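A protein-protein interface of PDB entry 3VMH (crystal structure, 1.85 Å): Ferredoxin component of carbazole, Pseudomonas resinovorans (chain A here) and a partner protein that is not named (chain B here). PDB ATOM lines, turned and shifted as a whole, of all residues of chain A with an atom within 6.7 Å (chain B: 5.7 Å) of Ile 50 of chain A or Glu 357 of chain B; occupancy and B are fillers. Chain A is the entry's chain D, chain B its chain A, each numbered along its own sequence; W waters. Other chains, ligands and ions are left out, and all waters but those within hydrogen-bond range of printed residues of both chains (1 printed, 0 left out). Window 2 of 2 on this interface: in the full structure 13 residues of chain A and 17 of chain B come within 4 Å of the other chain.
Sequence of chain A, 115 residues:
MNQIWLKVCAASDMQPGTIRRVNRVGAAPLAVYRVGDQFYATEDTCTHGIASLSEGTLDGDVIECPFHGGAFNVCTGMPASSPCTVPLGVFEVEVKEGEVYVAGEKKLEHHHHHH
N of His 48 of chain A sits close to SG of Cys 46 of chain A, at 3.5 Å. OD2 of Asp 359 of chain B lies within hydrogen-bond range of N of Phe 356 of chain B (2.9 Å).
N of Leu 355 of chain B touches O of His 48 of chain A (3.97 Å). Gly 49 of chain A touches Leu 355 of chain B (CA to O, 3.5 Å). Ile 50 of chain A touches Leu 355 of chain B (CG2 to O, 3.97 Å). Ile 50 of chain A touches Phe 356 of chain B (CG2 to C, 3.5 Å). Glu 357 of chain B touches Ile 50 of chain A (N to CG2, 3.8 Å). Ile 50 of chain A touches Asp 359 of chain B (CD1 to C, 3.9 Å). Ile 50 of chain A touches Glu 360 of chain B (CD1 to OE2, 3.6 Å). Ser 52 of chain A touches Arg 210 of chain B. Phe 67 of chain A touches Val 363 of chain B (CZ to CG1, 3.8 Å).
Of the printed residues of chain B, Gly 49 of chain A touches Leu 355. Of chain B, only Leu 355 (3.97 Å), Phe 356 (3.5 Å), Glu 357 (3.8 Å), Asp 359 (3.9 Å) and Glu 360 (3.6 Å) come within 4 Å of Ile 50 of chain A. Of the printed residues of chain B, Phe 67 of chain A touches Val 363. Of the printed residues of chain A, Asp 359 of chain B touches Ile 50. Printed residues of chain A within 4 Å of Val 363 of chain B: Phe 67 (3.8 Å). The nearest residue of chain B that does not touch Ile 50 of chain A is Val 363 of chain B (4.2 Å). The nearest residue of chain A that does not touch Glu 357 of chain B is Gly 49 of chain A (6.4 Å). The nearest printed residue of chain A that does not touch Phe 356 of chain B is Gly 49 of chain A (5.5 Å).
Of the 11 printed residues of chain B, 7 touch a printed residue of chain A. Printed residues of chain B that touch a printed residue of chain A: Arg 210, Leu 355, Phe 356, Glu 357, Asp 359, Glu 360 and Val 363. Hydrophobic or aromatic side chains of chain A that line the printed part of chain B: Ile 50 and Phe 67. Among the printed residues, 9 pairs touch across the chains.
Water W1 bridges the backbone carbonyl oxygen (O) of His 48 of chain A and the backbone NH (N) of Leu 355 of chain B.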
ATOM      1  N   THR A  45      21.110   2.596  15.543  1.00  0.00           N
ATOM      2  CA  THR A  45      21.471   2.359  14.154  1.00  0.00           C
ATOM      3  C   THR A  45      22.663   1.428  13.994  1.00  0.00           C
ATOM      4  O   THR A  45      23.728   1.654  14.567  1.00  0.00           O
ATOM      5  CB  THR A  45      21.786   3.683  13.443  1.00  0.00           C
ATOM      6  OG1 THR A  45      20.736   4.619  13.713  1.00  0.00           O
ATOM      7  CG2 THR A  45      21.884   3.470  11.936  1.00  0.00           C
ATOM      8  N   CYS A  46      22.471   0.374  13.208  1.00  0.00           N
ATOM      9  CA  CYS A  46      23.530  -0.589  12.950  1.00  0.00           C
ATOM     10  C   CYS A  46      24.666   0.135  12.234  1.00  0.00           C
ATOM     11  O   CYS A  46      24.424   0.902  11.300  1.00  0.00           O
ATOM     12  CB  CYS A  46      23.005  -1.725  12.072  1.00  0.00           C
ATOM     13  SG  CYS A  46      24.223  -2.999  11.732  1.00  0.00           S
ATOM     14  N   THR A  47      25.899  -0.108  12.671  1.00  0.00           N
ATOM     15  CA  THR A  47      27.064   0.541  12.076  1.00  0.00           C
ATOM     16  C   THR A  47      27.357   0.083  10.647  1.00  0.00           C
ATOM     17  O   THR A  47      28.149   0.714   9.935  1.00  0.00           O
ATOM     18  CB  THR A  47      28.336   0.313  12.924  1.00  0.00           C
ATOM     19  OG1 THR A  47      28.680  -1.078  12.917  1.00  0.00           O
ATOM     20  CG2 THR A  47      28.106   0.762  14.366  1.00  0.00           C
ATOM     21  N   HIS A  48      26.719  -1.002  10.224  1.00  0.00           N
ATOM     22  CA  HIS A  48      26.924  -1.531   8.878  1.00  0.00           C
ATOM     23  C   HIS A  48      25.962  -0.924   7.853  1.00  0.00           C
ATOM     24  O   HIS A  48      26.109  -1.135   6.648  1.00  0.00           O
ATOM     25  CB  HIS A  48      26.779  -3.061   8.899  1.00  0.00           C
ATOM     26  CG  HIS A  48      26.889  -3.707   7.550  1.00  0.00           C
ATOM     27  ND1 HIS A  48      25.796  -4.195   6.867  1.00  0.00           N
ATOM     28  CD2 HIS A  48      27.967  -3.968   6.771  1.00  0.00           C
ATOM     29  CE1 HIS A  48      26.195  -4.733   5.727  1.00  0.00           C
ATOM     30  NE2 HIS A  48      27.508  -4.609   5.645  1.00  0.00           N
ATOM     31  N   GLY A  49      24.978  -0.164   8.326  1.00  0.00           N
ATOM     32  CA  GLY A  49      24.026   0.430   7.405  1.00  0.00           C
ATOM     33  C   GLY A  49      23.129   1.481   8.018  1.00  0.00           C
ATOM     34  O   GLY A  49      23.604   2.441   8.625  1.00  0.00           O
ATOM     35  N   ILE A  50      21.825   1.297   7.855  1.00  0.00           N
ATOM     36  CA  ILE A  50      20.843   2.231   8.385  1.00  0.00           C
ATOM     37  C   ILE A  50      19.730   1.502   9.136  1.00  0.00           C
ATOM     38  O   ILE A  50      18.679   2.078   9.432  1.00  0.00           O
ATOM     39  CB  ILE A  50      20.226   3.079   7.248  1.00  0.00           C
ATOM     40  CG1 ILE A  50      19.609   2.172   6.177  1.00  0.00           C
ATOM     41  CG2 ILE A  50      21.304   3.957   6.625  1.00  0.00           C
ATOM     42  CD1 ILE A  50      18.945   2.932   5.027  1.00  0.00           C
ATOM     43  N   ALA A  51      19.972   0.235   9.453  1.00  0.00           N
ATOM     44  CA  ALA A  51      18.981  -0.569  10.162  1.00  0.00           C
ATOM     45  C   ALA A  51      18.816  -0.162  11.620  1.00  0.00           C
ATOM     46  O   ALA A  51      19.735   0.381  12.237  1.00  0.00           O
ATOM     47  CB  ALA A  51      19.366  -2.040  10.091  1.00  0.00           C
ATOM     48  N   SER A  52      17.629  -0.429  12.158  1.00  0.00           N
ATOM     49  CA  SER A  52      17.326  -0.140  13.552  1.00  0.00           C
ATOM     50  C   SER A  52      17.508  -1.448  14.316  1.00  0.00           C
ATOM     51  O   SER A  52      16.751  -2.395  14.121  1.00  0.00           O
ATOM     52  CB  SER A  52      15.882   0.350  13.698  1.00  0.00           C
ATOM     53  OG  SER A  52      15.494   0.400  15.065  1.00  0.00           O
ATOM     54  N   PHE A  67      18.566  -6.392   9.075  1.00  0.00           N
ATOM     55  CA  PHE A  67      18.929  -6.197   7.676  1.00  0.00           C
ATOM     56  C   PHE A  67      19.761  -7.307   7.053  1.00  0.00           C
ATOM     57  O   PHE A  67      19.321  -7.967   6.109  1.00  0.00           O
ATOM     58  CB  PHE A  67      19.684  -4.873   7.509  1.00  0.00           C
ATOM     59  CG  PHE A  67      18.795  -3.683   7.262  1.00  0.00           C
ATOM     60  CD1 PHE A  67      17.498  -3.634   7.769  1.00  0.00           C
ATOM     61  CD2 PHE A  67      19.279  -2.584   6.559  1.00  0.00           C
ATOM     62  CE1 PHE A  67      16.696  -2.502   7.579  1.00  0.00           C
ATOM     63  CE2 PHE A  67      18.486  -1.448   6.365  1.00  0.00           C
ATOM     64  CZ  PHE A  67      17.195  -1.409   6.877  1.00  0.00           C
ATOM     65  N   HIS A  68      20.964  -7.514   7.577  1.00  0.00           N
ATOM     66  CA  HIS A  68      21.850  -8.515   7.000  1.00  0.00           C
ATOM     67  C   HIS A  68      22.319  -9.612   7.939  1.00  0.00           C
ATOM     68  O   HIS A  68      23.126 -10.449   7.551  1.00  0.00           O
ATOM     69  CB  HIS A  68      23.060  -7.815   6.382  1.00  0.00           C
ATOM     70  CG  HIS A  68      22.701  -6.667   5.489  1.00  0.00           C
ATOM     71  ND1 HIS A  68      22.937  -5.353   5.833  1.00  0.00           N
ATOM     72  CD2 HIS A  68      22.115  -6.635   4.268  1.00  0.00           C
ATOM     73  CE1 HIS A  68      22.511  -4.561   4.866  1.00  0.00           C
ATOM     74  NE2 HIS A  68      22.008  -5.313   3.902  1.00  0.00           N
ATOM     75  N   PRO B 206      19.373  14.584   3.802  1.00  0.00           N
ATOM     76  CA  PRO B 206      18.087  14.255   4.427  1.00  0.00           C
ATOM     77  C   PRO B 206      17.693  15.118   5.619  1.00  0.00           C
ATOM     78  O   PRO B 206      18.544  15.569   6.380  1.00  0.00           O
ATOM     79  CB  PRO B 206      18.262  12.793   4.839  1.00  0.00           C
ATOM     80  CG  PRO B 206      19.253  12.272   3.855  1.00  0.00           C
ATOM     81  CD  PRO B 206      20.251  13.402   3.771  1.00  0.00           C
ATOM     82  N   ARG B 210      13.001   9.050   9.395  1.00  0.00           N
ATOM     83  CA  ARG B 210      13.050   8.067   8.317  1.00  0.00           C
ATOM     84  C   ARG B 210      11.665   7.805   7.739  1.00  0.00           C
ATOM     85  O   ARG B 210      11.521   7.564   6.542  1.00  0.00           O
ATOM     86  CB  ARG B 210      13.669   6.751   8.805  1.00  0.00           C
ATOM     87  CG  ARG B 210      12.822   5.960   9.786  1.00  0.00           C
ATOM     88  CD  ARG B 210      12.608   4.530   9.287  1.00  0.00           C
ATOM     89  NE  ARG B 210      13.111   3.529  10.226  1.00  0.00           N
ATOM     90  CZ  ARG B 210      12.944   2.215  10.087  1.00  0.00           C
ATOM     91  NH1 ARG B 210      12.282   1.735   9.041  1.00  0.00           N
ATOM     92  NH2 ARG B 210      13.438   1.380  10.992  1.00  0.00           N
ATOM     93  N   ILE B 231      12.518  12.296  -0.328  1.00  0.00           N
ATOM     94  CA  ILE B 231      13.742  12.827   0.260  1.00  0.00           C
ATOM     95  C   ILE B 231      13.829  14.354   0.125  1.00  0.00           C
ATOM     96  O   ILE B 231      14.422  15.023   0.973  1.00  0.00           O
ATOM     97  CB  ILE B 231      14.999  12.146  -0.364  1.00  0.00           C
ATOM     98  CG1 ILE B 231      16.219  12.386   0.528  1.00  0.00           C
ATOM     99  CG2 ILE B 231      15.245  12.672  -1.774  1.00  0.00           C
ATOM    100  CD1 ILE B 231      17.457  11.592   0.107  1.00  0.00           C
ATOM    101  N   LEU B 355      24.765   0.327   3.210  1.00  0.00           N
ATOM    102  CA  LEU B 355      23.812   1.368   2.845  1.00  0.00           C
ATOM    103  C   LEU B 355      23.981   2.675   3.619  1.00  0.00           C
ATOM    104  O   LEU B 355      24.539   2.684   4.713  1.00  0.00           O
ATOM    105  CB  LEU B 355      22.388   0.838   3.068  1.00  0.00           C
ATOM    106  CG  LEU B 355      22.084  -0.526   2.440  1.00  0.00           C
ATOM    107  CD1 LEU B 355      20.643  -0.918   2.724  1.00  0.00           C
ATOM    108  CD2 LEU B 355      22.337  -0.460   0.944  1.00  0.00           C
ATOM    109  N   PHE B 356      23.534   3.782   3.028  1.00  0.00           N
ATOM    110  CA  PHE B 356      23.577   5.050   3.740  1.00  0.00           C
ATOM    111  C   PHE B 356      22.184   5.678   3.686  1.00  0.00           C
ATOM    112  O   PHE B 356      21.260   5.074   3.139  1.00  0.00           O
ATOM    113  CB  PHE B 356      24.739   5.968   3.264  1.00  0.00           C
ATOM    114  CG  PHE B 356      24.533   6.671   1.952  1.00  0.00           C
ATOM    115  CD1 PHE B 356      23.921   6.048   0.869  1.00  0.00           C
ATOM    116  CD2 PHE B 356      25.082   7.945   1.770  1.00  0.00           C
ATOM    117  CE1 PHE B 356      23.866   6.678  -0.379  1.00  0.00           C
ATOM    118  CE2 PHE B 356      25.035   8.580   0.532  1.00  0.00           C
ATOM    119  CZ  PHE B 356      24.427   7.945  -0.549  1.00  0.00           C
ATOM    120  N   GLU B 357      22.018   6.860   4.270  1.00  0.00           N
ATOM    121  CA  GLU B 357      20.699   7.487   4.379  1.00  0.00           C
ATOM    122  C   GLU B 357      19.686   7.456   3.237  1.00  0.00           C
ATOM    123  O   GLU B 357      18.553   7.022   3.441  1.00  0.00           O
ATOM    124  CB  GLU B 357      20.857   8.928   4.881  1.00  0.00           C
ATOM    125  CG  GLU B 357      21.398   9.017   6.305  1.00  0.00           C
ATOM    126  CD  GLU B 357      22.913   8.877   6.389  1.00  0.00           C
ATOM    127  OE1 GLU B 357      23.573   8.777   5.335  1.00  0.00           O
ATOM    128  OE2 GLU B 357      23.446   8.879   7.522  1.00  0.00           O
ATOM    129  N   SER B 358      20.058   7.911   2.048  1.00  0.00           N
ATOM    130  CA  SER B 358      19.094   7.918   0.948  1.00  0.00           C
ATOM    131  C   SER B 358      18.584   6.530   0.553  1.00  0.00           C
ATOM    132  O   SER B 358      17.583   6.418  -0.151  1.00  0.00           O
ATOM    133  CB  SER B 358      19.686   8.626  -0.279  1.00  0.00           C
ATOM    134  OG  SER B 358      20.928   8.062  -0.646  1.00  0.00           O
ATOM    135  N   ASP B 359      19.261   5.476   1.002  1.00  0.00           N
ATOM    136  CA  ASP B 359      18.823   4.121   0.683  1.00  0.00           C
ATOM    137  C   ASP B 359      17.545   3.726   1.435  1.00  0.00           C
ATOM    138  O   ASP B 359      17.040   2.612   1.272  1.00  0.00           O
ATOM    139  CB  ASP B 359      19.941   3.107   0.965  1.00  0.00           C
ATOM    140  CG  ASP B 359      21.123   3.270   0.020  1.00  0.00           C
ATOM    141  OD1 ASP B 359      20.893   3.506  -1.186  1.00  0.00           O
ATOM    142  OD2 ASP B 359      22.277   3.158   0.479  1.00  0.00           O
ATOM    143  N   GLU B 360      17.020   4.630   2.258  1.00  0.00           N
ATOM    144  CA  GLU B 360      15.774   4.335   2.968  1.00  0.00           C
ATOM    145  C   GLU B 360      14.706   4.083   1.905  1.00  0.00           C
ATOM    146  O   GLU B 360      13.791   3.291   2.110  1.00  0.00           O
ATOM    147  CB  GLU B 360      15.337   5.512   3.852  1.00  0.00           C
ATOM    148  CG  GLU B 360      16.128   5.692   5.145  1.00  0.00           C
ATOM    149  CD  GLU B 360      15.896   4.574   6.162  1.00  0.00           C
ATOM    150  OE1 GLU B 360      15.021   3.710   5.929  1.00  0.00           O
ATOM    151  OE2 GLU B 360      16.592   4.572   7.206  1.00  0.00           O
ATOM    152  N   ALA B 361      14.832   4.761   0.764  1.00  0.00           N
ATOM    153  CA  ALA B 361      13.881   4.596  -0.334  1.00  0.00           C
ATOM    154  C   ALA B 361      13.948   3.170  -0.888  1.00  0.00           C
ATOM    155  O   ALA B 361      12.917   2.529  -1.120  1.00  0.00           O
ATOM    156  CB  ALA B 361      14.181   5.603  -1.445  1.00  0.00           C
ATOM    157  N   VAL B 363      15.138   0.500   0.672  1.00  0.00           N
ATOM    158  CA  VAL B 363      14.685  -0.414   1.718  1.00  0.00           C
ATOM    159  C   VAL B 363      13.149  -0.483   1.758  1.00  0.00           C
ATOM    160  O   VAL B 363      12.574  -1.563   1.919  1.00  0.00           O
ATOM    161  CB  VAL B 363      15.218   0.023   3.112  1.00  0.00           C
ATOM    162  CG1 VAL B 363      14.541  -0.787   4.215  1.00  0.00           C
ATOM    163  CG2 VAL B 363      16.724  -0.182   3.175  1.00  0.00           C
HETATM  164  O   HOH W   1      24.243  -1.922   4.805  1.00  0.00           O
